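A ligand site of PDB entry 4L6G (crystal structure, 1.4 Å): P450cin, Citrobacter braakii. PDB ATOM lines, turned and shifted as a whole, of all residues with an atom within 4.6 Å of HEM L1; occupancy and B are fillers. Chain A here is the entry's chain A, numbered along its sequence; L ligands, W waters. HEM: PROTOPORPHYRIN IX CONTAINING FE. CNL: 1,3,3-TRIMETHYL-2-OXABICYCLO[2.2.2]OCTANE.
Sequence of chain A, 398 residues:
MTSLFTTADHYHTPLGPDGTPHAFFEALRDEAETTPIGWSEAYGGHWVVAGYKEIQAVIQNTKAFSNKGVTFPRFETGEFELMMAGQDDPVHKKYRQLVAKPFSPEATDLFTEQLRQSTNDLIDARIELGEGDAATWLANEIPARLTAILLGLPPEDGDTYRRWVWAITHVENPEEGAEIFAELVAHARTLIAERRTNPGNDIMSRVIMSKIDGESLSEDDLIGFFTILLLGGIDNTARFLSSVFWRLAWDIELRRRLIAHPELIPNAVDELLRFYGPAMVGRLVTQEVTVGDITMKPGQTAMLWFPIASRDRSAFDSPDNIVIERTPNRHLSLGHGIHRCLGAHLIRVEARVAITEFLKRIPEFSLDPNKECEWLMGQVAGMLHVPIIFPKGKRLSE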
ATOM      1  N   ILE A  59      27.059   9.586  28.894  1.00  0.00           N
ATOM      2  CA  ILE A  59      26.488  10.920  28.776  1.00  0.00           C
ATOM      3  C   ILE A  59      25.116  10.976  29.485  1.00  0.00           C
ATOM      4  O   ILE A  59      24.697  12.046  29.918  1.00  0.00           O
ATOM      5  CB  ILE A  59      26.436  11.336  27.273  1.00  0.00           C
ATOM      6  CG1 ILE A  59      26.639  12.845  27.110  1.00  0.00           C
ATOM      7  CG2 ILE A  59      25.188  10.820  26.609  1.00  0.00           C
ATOM      8  CD1 ILE A  59      26.890  13.297  25.672  1.00  0.00           C
ATOM      9  N   ASN A  67      29.867  17.683  33.927  1.00  0.00           N
ATOM     10  CA  ASN A  67      30.243  18.643  32.898  1.00  0.00           C
ATOM     11  C   ASN A  67      31.275  19.681  33.341  1.00  0.00           C
ATOM     12  O   ASN A  67      31.674  20.544  32.532  1.00  0.00           O
ATOM     13  CB  ASN A  67      28.999  19.307  32.325  1.00  0.00           C
ATOM     14  CG  ASN A  67      28.506  18.579  31.105  1.00  0.00           C
ATOM     15  OD1 ASN A  67      28.229  17.366  31.187  1.00  0.00           O
ATOM     16  ND2 ASN A  67      28.494  19.248  29.958  1.00  0.00           N
ATOM     17  N   VAL A  70      33.805  19.434  30.702  1.00  0.00           N
ATOM     18  CA  VAL A  70      33.294  19.526  29.330  1.00  0.00           C
ATOM     19  C   VAL A  70      34.398  19.831  28.307  1.00  0.00           C
ATOM     20  O   VAL A  70      34.391  19.274  27.213  1.00  0.00           O
ATOM     21  CB  VAL A  70      32.149  20.560  29.202  1.00  0.00           C
ATOM     22  CG1 VAL A  70      32.618  21.951  29.617  1.00  0.00           C
ATOM     23  CG2 VAL A  70      31.519  20.529  27.784  1.00  0.00           C
ATOM     24  N   MET A  84      25.874  26.761  31.306  1.00  0.00           N
ATOM     25  CA  MET A  84      25.123  25.580  30.890  1.00  0.00           C
ATOM     26  C   MET A  84      26.063  24.420  30.615  1.00  0.00           C
ATOM     27  O   MET A  84      26.020  23.428  31.333  1.00  0.00           O
ATOM     28  CB  MET A  84      24.238  25.892  29.667  1.00  0.00           C
ATOM     29  CG  MET A  84      23.191  26.999  29.983  1.00  0.00           C
ATOM     30  SD  MET A  84      22.399  27.617  28.485  1.00  0.00           S
ATOM     31  CE  MET A  84      23.705  28.641  27.809  1.00  0.00           C
ATOM     32  N   ALA A  85      26.930  24.541  29.609  1.00  0.00           N
ATOM     33  CA  ALA A  85      27.786  23.432  29.208  1.00  0.00           C
ATOM     34  C   ALA A  85      28.777  23.046  30.297  1.00  0.00           C
ATOM     35  O   ALA A  85      29.208  21.893  30.349  1.00  0.00           O
ATOM     36  CB  ALA A  85      28.533  23.753  27.924  1.00  0.00           C
ATOM     37  N   HIS A  92      22.547  23.911  36.188  1.00  0.00           N
ATOM     38  CA  HIS A  92      22.448  23.851  34.748  1.00  0.00           C
ATOM     39  C   HIS A  92      21.030  24.119  34.240  1.00  0.00           C
ATOM     40  O   HIS A  92      20.801  24.928  33.342  1.00  0.00           O
ATOM     41  CB  HIS A  92      22.924  22.482  34.260  1.00  0.00           C
ATOM     42  CG  HIS A  92      22.431  22.127  32.903  1.00  0.00           C
ATOM     43  ND1 HIS A  92      21.323  21.347  32.690  1.00  0.00           N
ATOM     44  CD2 HIS A  92      22.878  22.477  31.672  1.00  0.00           C
ATOM     45  CE1 HIS A  92      21.115  21.199  31.393  1.00  0.00           C
ATOM     46  NE2 HIS A  92      22.053  21.878  30.747  1.00  0.00           N
ATOM     47  N   ARG A  96      19.788  27.210  31.758  1.00  0.00           N
ATOM     48  CA  ARG A  96      19.333  26.902  30.410  1.00  0.00           C
ATOM     49  C   ARG A  96      17.912  27.414  30.190  1.00  0.00           C
ATOM     50  O   ARG A  96      17.600  27.908  29.117  1.00  0.00           O
ATOM     51  CB  ARG A  96      19.406  25.395  30.104  1.00  0.00           C
ATOM     52  CG  ARG A  96      18.979  25.080  28.674  1.00  0.00           C
ATOM     53  CD  ARG A  96      19.265  23.638  28.287  1.00  0.00           C
ATOM     54  NE  ARG A  96      18.693  23.320  26.985  1.00  0.00           N
ATOM     55  CZ  ARG A  96      19.287  22.564  26.070  1.00  0.00           C
ATOM     56  NH1 ARG A  96      20.488  22.055  26.324  1.00  0.00           N
ATOM     57  NH2 ARG A  96      18.686  22.330  24.910  1.00  0.00           N
ATOM     58  N   PHE A 103      16.118  30.361  21.588  1.00  0.00           N
ATOM     59  CA  PHE A 103      16.672  29.328  20.737  1.00  0.00           C
ATOM     60  C   PHE A 103      15.610  28.359  20.240  1.00  0.00           C
ATOM     61  O   PHE A 103      15.924  27.382  19.558  1.00  0.00           O
ATOM     62  CB  PHE A 103      17.790  28.585  21.465  1.00  0.00           C
ATOM     63  CG  PHE A 103      19.059  29.370  21.512  1.00  0.00           C
ATOM     64  CD1 PHE A 103      19.898  29.408  20.418  1.00  0.00           C
ATOM     65  CD2 PHE A 103      19.369  30.142  22.616  1.00  0.00           C
ATOM     66  CE1 PHE A 103      21.055  30.155  20.437  1.00  0.00           C
ATOM     67  CE2 PHE A 103      20.532  30.890  22.643  1.00  0.00           C
ATOM     68  CZ  PHE A 103      21.370  30.900  21.551  1.00  0.00           C
ATOM     69  N   LEU A 150      22.889  37.975  17.529  1.00  0.00           N
ATOM     70  CA  LEU A 150      22.332  37.353  18.737  1.00  0.00           C
ATOM     71  C   LEU A 150      22.826  38.001  20.021  1.00  0.00           C
ATOM     72  O   LEU A 150      22.096  38.055  21.021  1.00  0.00           O
ATOM     73  CB  LEU A 150      22.667  35.858  18.796  1.00  0.00           C
ATOM     74  CG  LEU A 150      22.097  34.901  17.762  1.00  0.00           C
ATOM     75  CD1 LEU A 150      22.588  33.479  18.040  1.00  0.00           C
ATOM     76  CD2 LEU A 150      20.581  34.980  17.836  1.00  0.00           C
ATOM     77  N   ILE A 228      30.022  31.213  25.854  1.00  0.00           N
ATOM     78  CA  ILE A 228      29.607  29.959  25.223  1.00  0.00           C
ATOM     79  C   ILE A 228      28.828  30.203  23.939  1.00  0.00           C
ATOM     80  O   ILE A 228      28.964  29.456  22.970  1.00  0.00           O
ATOM     81  CB  ILE A 228      28.765  29.035  26.179  1.00  0.00           C
ATOM     82  CG1 ILE A 228      28.518  27.694  25.480  1.00  0.00           C
ATOM     83  CG2 ILE A 228      27.441  29.692  26.611  1.00  0.00           C
ATOM     84  CD1 ILE A 228      27.935  26.655  26.341  1.00  0.00           C
ATOM     85  N   LEU A 229      28.061  31.277  23.896  1.00  0.00           N
ATOM     86  CA  LEU A 229      27.290  31.555  22.691  1.00  0.00           C
ATOM     87  C   LEU A 229      28.224  32.019  21.575  1.00  0.00           C
ATOM     88  O   LEU A 229      28.044  31.668  20.425  1.00  0.00           O
ATOM     89  CB  LEU A 229      26.197  32.579  23.006  1.00  0.00           C
ATOM     90  CG  LEU A 229      25.229  32.140  24.133  1.00  0.00           C
ATOM     91  CD1 LEU A 229      24.221  33.222  24.533  1.00  0.00           C
ATOM     92  CD2 LEU A 229      24.499  30.834  23.767  1.00  0.00           C
ATOM     93  N   GLY A 232      29.876  28.749  20.178  1.00  0.00           N
ATOM     94  CA  GLY A 232      28.977  27.996  19.310  1.00  0.00           C
ATOM     95  C   GLY A 232      28.968  28.448  17.849  1.00  0.00           C
ATOM     96  O   GLY A 232      28.984  27.621  16.932  1.00  0.00           O
ATOM     97  N   GLY A 233      28.967  29.753  17.630  1.00  0.00           N
ATOM     98  CA  GLY A 233      28.970  30.297  16.268  1.00  0.00           C
ATOM     99  C   GLY A 233      30.336  30.337  15.596  1.00  0.00           C
ATOM    100  O   GLY A 233      30.564  29.747  14.532  1.00  0.00           O
ATOM    101  N   ASN A 236      32.297  26.304  16.453  1.00  0.00           N
ATOM    102  CA  ASN A 236      31.631  25.087  16.014  1.00  0.00           C
ATOM    103  C   ASN A 236      30.994  25.215  14.632  1.00  0.00           C
ATOM    104  O   ASN A 236      31.230  24.391  13.754  1.00  0.00           O
ATOM    105  CB  ASN A 236      30.565  24.673  17.025  1.00  0.00           C
ATOM    106  CG  ASN A 236      31.129  24.481  18.437  1.00  0.00           C
ATOM    107  OD1 ASN A 236      32.159  25.044  18.811  1.00  0.00           O
ATOM    108  ND2 ASN A 236      30.440  23.699  19.229  1.00  0.00           N
ATOM    109  N   THR A 237      30.184  26.238  14.437  1.00  0.00           N
ATOM    110  CA  THR A 237      29.448  26.348  13.201  1.00  0.00           C
ATOM    111  C   THR A 237      30.370  26.615  12.014  1.00  0.00           C
ATOM    112  O   THR A 237      30.217  26.041  10.939  1.00  0.00           O
ATOM    113  CB  THR A 237      28.376  27.446  13.301  1.00  0.00           C
ATOM    114  OG1 THR A 237      27.558  27.182  14.437  1.00  0.00           O
ATOM    115  CG2 THR A 237      27.505  27.414  12.056  1.00  0.00           C
ATOM    116  N   PHE A 240      32.181  23.394  11.005  1.00  0.00           N
ATOM    117  CA  PHE A 240      31.257  22.493  10.309  1.00  0.00           C
ATOM    118  C   PHE A 240      30.994  22.964   8.881  1.00  0.00           C
ATOM    119  O   PHE A 240      31.158  22.194   7.917  1.00  0.00           O
ATOM    120  CB  PHE A 240      29.939  22.402  11.083  1.00  0.00           C
ATOM    121  CG  PHE A 240      28.861  21.643  10.356  1.00  0.00           C
ATOM    122  CD1 PHE A 240      27.673  22.265  10.016  1.00  0.00           C
ATOM    123  CD2 PHE A 240      29.068  20.328   9.972  1.00  0.00           C
ATOM    124  CE1 PHE A 240      26.669  21.582   9.319  1.00  0.00           C
ATOM    125  CE2 PHE A 240      28.080  19.621   9.265  1.00  0.00           C
ATOM    126  CZ  PHE A 240      26.869  20.246   8.941  1.00  0.00           C
ATOM    127  N   LEU A 273      26.171  16.551   9.289  1.00  0.00           N
ATOM    128  CA  LEU A 273      26.443  16.697  10.713  1.00  0.00           C
ATOM    129  C   LEU A 273      26.971  15.406  11.329  1.00  0.00           C
ATOM    130  O   LEU A 273      27.877  15.439  12.168  1.00  0.00           O
ATOM    131  CB  LEU A 273      25.199  17.141  11.477  1.00  0.00           C
ATOM    132  CG  LEU A 273      24.969  18.639  11.625  1.00  0.00           C
ATOM    133  CD1 LEU A 273      23.630  18.851  12.269  1.00  0.00           C
ATOM    134  CD2 LEU A 273      26.082  19.305  12.466  1.00  0.00           C
ATOM    135  N   PRO A 278      31.931  18.617  14.172  1.00  0.00           N
ATOM    136  CA  PRO A 278      33.262  18.990  14.621  1.00  0.00           C
ATOM    137  C   PRO A 278      33.568  18.648  16.088  1.00  0.00           C
ATOM    138  O   PRO A 278      34.737  18.642  16.469  1.00  0.00           O
ATOM    139  CB  PRO A 278      33.287  20.514  14.413  1.00  0.00           C
ATOM    140  CG  PRO A 278      31.884  20.926  14.382  1.00  0.00           C
ATOM    141  CD  PRO A 278      31.106  19.784  13.811  1.00  0.00           C
ATOM    142  N   ALA A 279      32.551  18.371  16.899  1.00  0.00           N
ATOM    143  CA  ALA A 279      32.731  18.426  18.355  1.00  0.00           C
ATOM    144  C   ALA A 279      33.049  17.096  19.024  1.00  0.00           C
ATOM    145  O   ALA A 279      32.594  16.025  18.613  1.00  0.00           O
ATOM    146  CB  ALA A 279      31.484  19.005  19.018  1.00  0.00           C
ATOM    147  N   VAL A 281      33.385  16.132  23.493  1.00  0.00           N
ATOM    148  CA  VAL A 281      33.262  16.723  24.827  1.00  0.00           C
ATOM    149  C   VAL A 281      33.895  15.799  25.847  1.00  0.00           C
ATOM    150  O   VAL A 281      33.992  14.581  25.624  1.00  0.00           O
ATOM    151  CB  VAL A 281      31.793  17.005  25.265  1.00  0.00           C
ATOM    152  CG1 VAL A 281      31.112  17.981  24.316  1.00  0.00           C
ATOM    153  CG2 VAL A 281      30.984  15.703  25.424  1.00  0.00           C
ATOM    154  N   ARG A 283      34.087  14.583  30.169  1.00  0.00           N
ATOM    155  CA  ARG A 283      33.351  14.430  31.415  1.00  0.00           C
ATOM    156  C   ARG A 283      34.360  14.157  32.511  1.00  0.00           C
ATOM    157  O   ARG A 283      35.295  13.372  32.313  1.00  0.00           O
ATOM    158  CB  ARG A 283      32.336  13.272  31.346  1.00  0.00           C
ATOM    159  CG  ARG A 283      31.196  13.482  30.333  1.00  0.00           C
ATOM    160  CD  ARG A 283      30.266  14.605  30.762  1.00  0.00           C
ATOM    161  NE  ARG A 283      29.046  14.721  29.946  1.00  0.00           N
ATOM    162  CZ  ARG A 283      28.866  15.584  28.949  1.00  0.00           C
ATOM    163  NH1 ARG A 283      29.862  16.354  28.504  1.00  0.00           N
ATOM    164  NH2 ARG A 283      27.672  15.653  28.362  1.00  0.00           N
ATOM    165  N   PHE A 306      32.664  11.537  19.781  1.00  0.00           N
ATOM    166  CA  PHE A 306      31.462  11.489  18.957  1.00  0.00           C
ATOM    167  C   PHE A 306      31.723  11.072  17.506  1.00  0.00           C
ATOM    168  O   PHE A 306      30.934  10.296  16.967  1.00  0.00           O
ATOM    169  CB  PHE A 306      30.748  12.834  18.966  1.00  0.00           C
ATOM    170  CG  PHE A 306      30.210  13.266  20.307  1.00  0.00           C
ATOM    171  CD1 PHE A 306      30.202  14.609  20.646  1.00  0.00           C
ATOM    172  CD2 PHE A 306      29.635  12.356  21.182  1.00  0.00           C
ATOM    173  CE1 PHE A 306      29.665  15.065  21.851  1.00  0.00           C
ATOM    174  CE2 PHE A 306      29.079  12.785  22.388  1.00  0.00           C
ATOM    175  CZ  PHE A 306      29.095  14.147  22.722  1.00  0.00           C
ATOM    176  N   SER A 333      26.481  14.138  17.126  1.00  0.00           N
ATOM    177  CA  SER A 333      27.239  15.355  16.847  1.00  0.00           C
ATOM    178  C   SER A 333      26.778  16.570  17.638  1.00  0.00           C
ATOM    179  O   SER A 333      27.555  17.533  17.835  1.00  0.00           O
ATOM    180  CB  SER A 333      27.191  15.651  15.358  1.00  0.00           C
ATOM    181  OG  SER A 333      27.872  14.628  14.649  1.00  0.00           O
ATOM    182  N   LEU A 334      25.517  16.555  18.074  1.00  0.00           N
ATOM    183  CA  LEU A 334      24.978  17.636  18.901  1.00  0.00           C
ATOM    184  C   LEU A 334      24.797  17.201  20.350  1.00  0.00           C
ATOM    185  O   LEU A 334      24.117  17.874  21.120  1.00  0.00           O
ATOM    186  CB  LEU A 334      23.625  18.137  18.350  1.00  0.00           C
ATOM    187  CG  LEU A 334      23.673  18.667  16.919  1.00  0.00           C
ATOM    188  CD1 LEU A 334      22.295  19.032  16.428  1.00  0.00           C
ATOM    189  CD2 LEU A 334      24.631  19.850  16.818  1.00  0.00           C
ATOM    190  N   GLY A 335      25.453  16.104  20.732  1.00  0.00           N
ATOM    191  CA  GLY A 335      25.307  15.574  22.073  1.00  0.00           C
ATOM    192  C   GLY A 335      24.031  14.765  22.265  1.00  0.00           C
ATOM    193  O   GLY A 335      23.398  14.293  21.295  1.00  0.00           O
ATOM    194  N   ILE A 338      20.812  15.832  28.837  1.00  0.00           N
ATOM    195  CA  ILE A 338      20.414  17.141  29.345  1.00  0.00           C
ATOM    196  C   ILE A 338      21.220  18.310  28.763  1.00  0.00           C
ATOM    197  O   ILE A 338      20.730  19.449  28.766  1.00  0.00           O
ATOM    198  CB  ILE A 338      20.459  17.178  30.898  1.00  0.00           C
ATOM    199  CG1 ILE A 338      21.904  17.043  31.407  1.00  0.00           C
ATOM    200  CG2 ILE A 338      19.559  16.078  31.471  1.00  0.00           C
ATOM    201  CD1 ILE A 338      22.081  17.434  32.865  1.00  0.00           C
ATOM    202  N   HIS A 339      22.412  18.051  28.227  1.00  0.00           N
ATOM    203  CA  HIS A 339      23.223  19.112  27.633  1.00  0.00           C
ATOM    204  C   HIS A 339      23.127  19.201  26.099  1.00  0.00           C
ATOM    205  O   HIS A 339      23.890  19.951  25.490  1.00  0.00           O
ATOM    206  CB  HIS A 339      24.700  18.944  28.009  1.00  0.00           C
ATOM    207  CG  HIS A 339      24.967  19.108  29.473  1.00  0.00           C
ATOM    208  ND1 HIS A 339      25.046  20.353  30.074  1.00  0.00           N
ATOM    209  CD2 HIS A 339      25.184  18.200  30.457  1.00  0.00           C
ATOM    210  CE1 HIS A 339      25.264  20.194  31.375  1.00  0.00           C
ATOM    211  NE2 HIS A 339      25.368  18.893  31.629  1.00  0.00           N
ATOM    212  N   ARG A 340      22.184  18.465  25.497  1.00  0.00           N
ATOM    213  CA  ARG A 340      22.091  18.418  24.039  1.00  0.00           C
ATOM    214  C   ARG A 340      22.005  19.841  23.459  1.00  0.00           C
ATOM    215  O   ARG A 340      21.265  20.669  23.996  1.00  0.00           O
ATOM    216  CB  ARG A 340      20.898  17.566  23.570  1.00  0.00           C
ATOM    217  CG  ARG A 340      20.962  17.243  22.072  1.00  0.00           C
ATOM    218  CD  ARG A 340      19.861  16.294  21.614  1.00  0.00           C
ATOM    219  NE  ARG A 340      19.992  15.924  20.206  1.00  0.00           N
ATOM    220  CZ  ARG A 340      19.502  16.641  19.202  1.00  0.00           C
ATOM    221  NH1 ARG A 340      18.885  17.781  19.467  1.00  0.00           N
ATOM    222  NH2 ARG A 340      19.679  16.260  17.945  1.00  0.00           N
ATOM    223  N   CYS A 341      22.771  20.093  22.410  1.00  0.00           N
ATOM    224  CA  CYS A 341      22.986  21.434  21.839  1.00  0.00           C
ATOM    225  C   CYS A 341      21.776  22.355  21.836  1.00  0.00           C
ATOM    226  O   CYS A 341      20.751  22.071  21.226  1.00  0.00           O
ATOM    227  CB  CYS A 341      23.508  21.316  20.412  1.00  0.00           C
ATOM    228  SG  CYS A 341      23.907  22.916  19.663  1.00  0.00           S
ATOM    229  N   LEU A 342      21.929  23.480  22.523  1.00  0.00           N
ATOM    230  CA  LEU A 342      20.929  24.518  22.549  1.00  0.00           C
ATOM    231  C   LEU A 342      20.692  25.124  21.147  1.00  0.00           C
ATOM    232  O   LEU A 342      19.591  25.577  20.799  1.00  0.00           O
ATOM    233  CB  LEU A 342      21.373  25.587  23.547  1.00  0.00           C
ATOM    234  CG  LEU A 342      20.441  26.299  24.532  1.00  0.00           C
ATOM    235  CD1 LEU A 342      20.845  27.763  24.573  1.00  0.00           C
ATOM    236  CD2 LEU A 342      18.978  26.117  24.233  1.00  0.00           C
ATOM    237  N   GLY A 343      21.745  25.159  20.355  1.00  0.00           N
ATOM    238  CA  GLY A 343      21.672  25.784  19.044  1.00  0.00           C
ATOM    239  C   GLY A 343      21.272  24.872  17.912  1.00  0.00           C
ATOM    240  O   GLY A 343      21.410  25.261  16.753  1.00  0.00           O
ATOM    241  N   LEU A 346      19.013  26.300  15.184  1.00  0.00           N
ATOM    242  CA  LEU A 346      19.661  27.438  14.544  1.00  0.00           C
ATOM    243  C   LEU A 346      20.718  26.985  13.520  1.00  0.00           C
ATOM    244  O   LEU A 346      20.777  27.502  12.389  1.00  0.00           O
ATOM    245  CB  LEU A 346      20.292  28.351  15.597  1.00  0.00           C
ATOM    246  CG  LEU A 346      20.993  29.594  15.064  1.00  0.00           C
ATOM    247  CD1 LEU A 346      20.047  30.492  14.282  1.00  0.00           C
ATOM    248  CD2 LEU A 346      21.615  30.357  16.203  1.00  0.00           C
ATOM    249  N   ILE A 347      21.537  26.005  13.892  1.00  0.00           N
ATOM    250  CA  ILE A 347      22.593  25.616  12.953  1.00  0.00           C
ATOM    251  C   ILE A 347      21.984  24.875  11.755  1.00  0.00           C
ATOM    252  O   ILE A 347      22.508  24.966  10.638  1.00  0.00           O
ATOM    253  CB  ILE A 347      23.677  24.787  13.647  1.00  0.00           C
ATOM    254  CG1 ILE A 347      23.175  23.407  14.043  1.00  0.00           C
ATOM    255  CG2 ILE A 347      24.206  25.539  14.841  1.00  0.00           C
ATOM    256  CD1 ILE A 347      23.685  22.327  13.114  1.00  0.00           C
HETATM  257  CHA HEM L   1      25.890  22.026  23.664  1.00  0.00           C
HETATM  258  CHB HEM L   1      27.819  20.801  19.363  1.00  0.00           C
HETATM  259  CHC HEM L   1      26.563  25.129  17.499  1.00  0.00           C
HETATM  260  CHD HEM L   1      25.144  26.551  21.908  1.00  0.00           C
HETATM  261  C1A HEM L   1      26.474  21.311  22.644  1.00  0.00           C
HETATM  262  C2A HEM L   1      26.956  19.947  22.754  1.00  0.00           C
HETATM  263  C3A HEM L   1      27.490  19.626  21.559  1.00  0.00           C
HETATM  264  C4A HEM L   1      27.380  20.770  20.675  1.00  0.00           C
HETATM  265  CMA HEM L   1      28.158  18.289  21.178  1.00  0.00           C
HETATM  266  CAA HEM L   1      26.810  19.040  24.011  1.00  0.00           C
HETATM  267  CBA HEM L   1      27.767  19.425  25.120  1.00  0.00           C
HETATM  268  CGA HEM L   1      27.961  18.329  26.140  1.00  0.00           C
HETATM  269  O1A HEM L   1      27.371  17.214  26.049  1.00  0.00           O
HETATM  270  O2A HEM L   1      28.714  18.601  27.104  1.00  0.00           O
HETATM  271  C1B HEM L   1      27.598  21.840  18.487  1.00  0.00           C
HETATM  272  C2B HEM L   1      27.883  21.815  17.066  1.00  0.00           C
HETATM  273  C3B HEM L   1      27.546  23.010  16.551  1.00  0.00           C
HETATM  274  C4B HEM L   1      27.049  23.831  17.640  1.00  0.00           C
HETATM  275  CMB HEM L   1      28.494  20.590  16.352  1.00  0.00           C
HETATM  276  CAB HEM L   1      27.616  23.536  15.104  1.00  0.00           C
HETATM  277  CBB HEM L   1      27.705  22.763  14.035  1.00  0.00           C
HETATM  278  C1C HEM L   1      26.063  25.897  18.531  1.00  0.00           C
HETATM  279  C2C HEM L   1      25.580  27.261  18.421  1.00  0.00           C
HETATM  280  C3C HEM L   1      25.184  27.647  19.650  1.00  0.00           C
HETATM  281  C4C HEM L   1      25.424  26.540  20.564  1.00  0.00           C
HETATM  282  CMC HEM L   1      25.545  28.038  17.090  1.00  0.00           C
HETATM  283  CAC HEM L   1      24.603  28.987  20.129  1.00  0.00           C
HETATM  284  CBC HEM L   1      24.726  30.141  19.459  1.00  0.00           C
HETATM  285  C1D HEM L   1      25.276  25.490  22.787  1.00  0.00           C
HETATM  286  C2D HEM L   1      25.064  25.575  24.215  1.00  0.00           C
HETATM  287  C3D HEM L   1      25.297  24.184  24.774  1.00  0.00           C
HETATM  288  C4D HEM L   1      25.621  23.375  23.624  1.00  0.00           C
HETATM  289  CMD HEM L   1      24.692  26.821  25.015  1.00  0.00           C
HETATM  290  CAD HEM L   1      25.186  23.747  26.247  1.00  0.00           C
HETATM  291  CBD HEM L   1      23.737  23.322  26.475  1.00  0.00           C
HETATM  292  CGD HEM L   1      23.570  22.733  27.859  1.00  0.00           C
HETATM  293  O1D HEM L   1      22.418  22.438  28.250  1.00  0.00           O
HETATM  294  O2D HEM L   1      24.605  22.530  28.527  1.00  0.00           O
HETATM  295  NA  HEM L   1      26.726  21.783  21.364  1.00  0.00           N
HETATM  296  NB  HEM L   1      27.104  23.098  18.820  1.00  0.00           N
HETATM  297  NC  HEM L   1      25.935  25.478  19.855  1.00  0.00           N
HETATM  298  ND  HEM L   1      25.616  24.172  22.467  1.00  0.00           N
HETATM  299 FE   HEM L   1      26.088  23.549  20.564  1.00  0.00          FE
HETATM  300  C1  CNL L   2      30.452  24.528  23.029  1.00  0.00           C
HETATM  301  C2  CNL L   2      29.386  23.740  23.721  1.00  0.00           C
HETATM  302  C3  CNL L   2      29.941  22.594  24.485  1.00  0.00           C
HETATM  303  C4  CNL L   2      31.407  22.447  24.314  1.00  0.00           C
HETATM  304  C5  CNL L   2      32.039  23.669  24.716  1.00  0.00           C
HETATM  305  C6  CNL L   2      31.529  24.888  24.004  1.00  0.00           C
HETATM  306  C7  CNL L   2      29.916  25.697  22.300  1.00  0.00           C
HETATM  307  C8  CNL L   2      31.639  22.313  22.824  1.00  0.00           C
HETATM  308  C9  CNL L   2      30.979  21.124  22.195  1.00  0.00           C
HETATM  309  C10 CNL L   2      33.093  22.186  22.452  1.00  0.00           C
HETATM  310  O   CNL L   2      31.020  23.552  22.103  1.00  0.00           O
HETATM  311  O   HOH W   1      29.856  17.454  16.327  1.00  0.00           O
HETATM  312  O   HOH W   2      24.897  16.336  25.414  1.00  0.00           O
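An iron atom (FE) of HEM L1 is bound by the side-chain sulfur of Cys 341, at 2.4 Å.
A ring nitrogen (NE2) of His 92 sits at hydrogen-bond distance from an oxygen (O1D) of HEM L1, 2.6 Å away.
A ring nitrogen (ND1) of His 339 lies within hydrogen-bond range of an oxygen (O2D) of HEM L1 (2.7 Å).
The guanidinium group (NH1) of Arg 96 lies within salt-bridge range of an oxygen (O1D) of HEM L1.
NH2 of Arg 283 lies within salt-bridge range of O1A of HEM L1 (2.8 Å).
An oxygen (O2A) of HEM L1 sits at hydrogen-bond distance from the side-chain amide nitrogen (ND2) of Asn 67, at 2.9 Å.
The backbone NH of Ala 85 is in hydrogen-bond range of an oxygen (O2D) of HEM L1, at 3.3 Å.
An oxygen (O) of CNL L2 sits at hydrogen-bond distance from the side-chain amide nitrogen (ND2) of Asn 236 (2.9 Å).
O of Leu 334 sits at hydrogen-bond distance from N of Cys 341, at 2.9 Å.
SG of Cys 341 lies close to N of Gly 343.
NE2 of His 92 sits close to O of Ile 338 (3.4 Å).
The side-chain amide oxygen (OD1) of Asn 67 sits close to a ring nitrogen (NE2) of His 339, 3.3 Å away.
The backbone carbonyl oxygen of Met 84 lies close to a ring nitrogen (ND1) of His 339.
The guanidinium group (NH1) of Arg 96 sits at hydrogen-bond distance from the backbone carbonyl oxygen (O) of Arg 340 (2.8 Å).
The guanidinium group (NE) of Arg 283 lies close to the side-chain amide oxygen (OD1) of Asn 67.
The backbone carbonyl oxygen (O) of Gly 232 is in hydrogen-bond range of the side-chain hydroxyl (OG1) of Thr 237, 2.9 Å away.
O2D of HEM L1 sits close to O of Met 84 (3.3 Å).
The side-chain amide nitrogen of Asn 236 lies close to a nitrogen (NB) of HEM L1, 3.4 Å away.
O of Ile 338 sits close to O1D of HEM L1 (3.5 Å).
Ile 59 touches HEM L1 (CD1 to O1A, 3.96 Å).
Val 70 touches HEM L1.
Phe 103 touches HEM L1 (CE1 to CAC, 3.7 Å).
CD1 of Ile 228 touches CMD of HEM L1 (3.5 Å).
Leu 229 touches HEM L1 (O to CBC, 3.8 Å).
Gly 232 touches HEM L1 (O to CMC, 3.5 Å).
Gly 233 touches HEM L1.
Thr 237 touches HEM L1 (OG1 to CMC, 3.4 Å).
CB of Phe 240 touches CBB of HEM L1 (3.7 Å).
CD of Pro 278 touches CMB of HEM L1, 3.7 Å away.
Val 281 touches HEM L1 (CG1 to CGA, 3.7 Å).
CE1 of Phe 306 touches CMA of HEM L1 (3.6 Å).
Ser 333 touches HEM L1.
Leu 334 touches HEM L1 (C to CMA, 3.6 Å).
Gly 335 touches HEM L1.
CB of Leu 342 touches C2D of HEM L1, at 3.8 Å.
Gly 343 touches HEM L1 (N to C4C, 3.9 Å).
Ile 347 touches HEM L1 (CG2 to CHC, 3.6 Å).
Hydrophobic or aromatic side chains within 4 Å of HEM L1: Ile 59, Val 70, Met 84, Ala 85, His 92, Phe 103, Ile 228, Phe 240, Pro 278, Val 281, Phe 306, Leu 334, His 339, Leu 342 and Ile 347.
The nearest printed residue that does not touch HEM L1 is Ala 279 (4.03 Å).
Water W2 lies within hydrogen-bond range of an oxygen (O1A) of HEM L1 and the backbone NH of Arg 340.
Water W1 lies within hydrogen-bond range of the backbone carbonyl oxygen (O) of Ser 333 (2.8 Å) and the backbone NH (N) of Ala 279 (2.9 Å).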
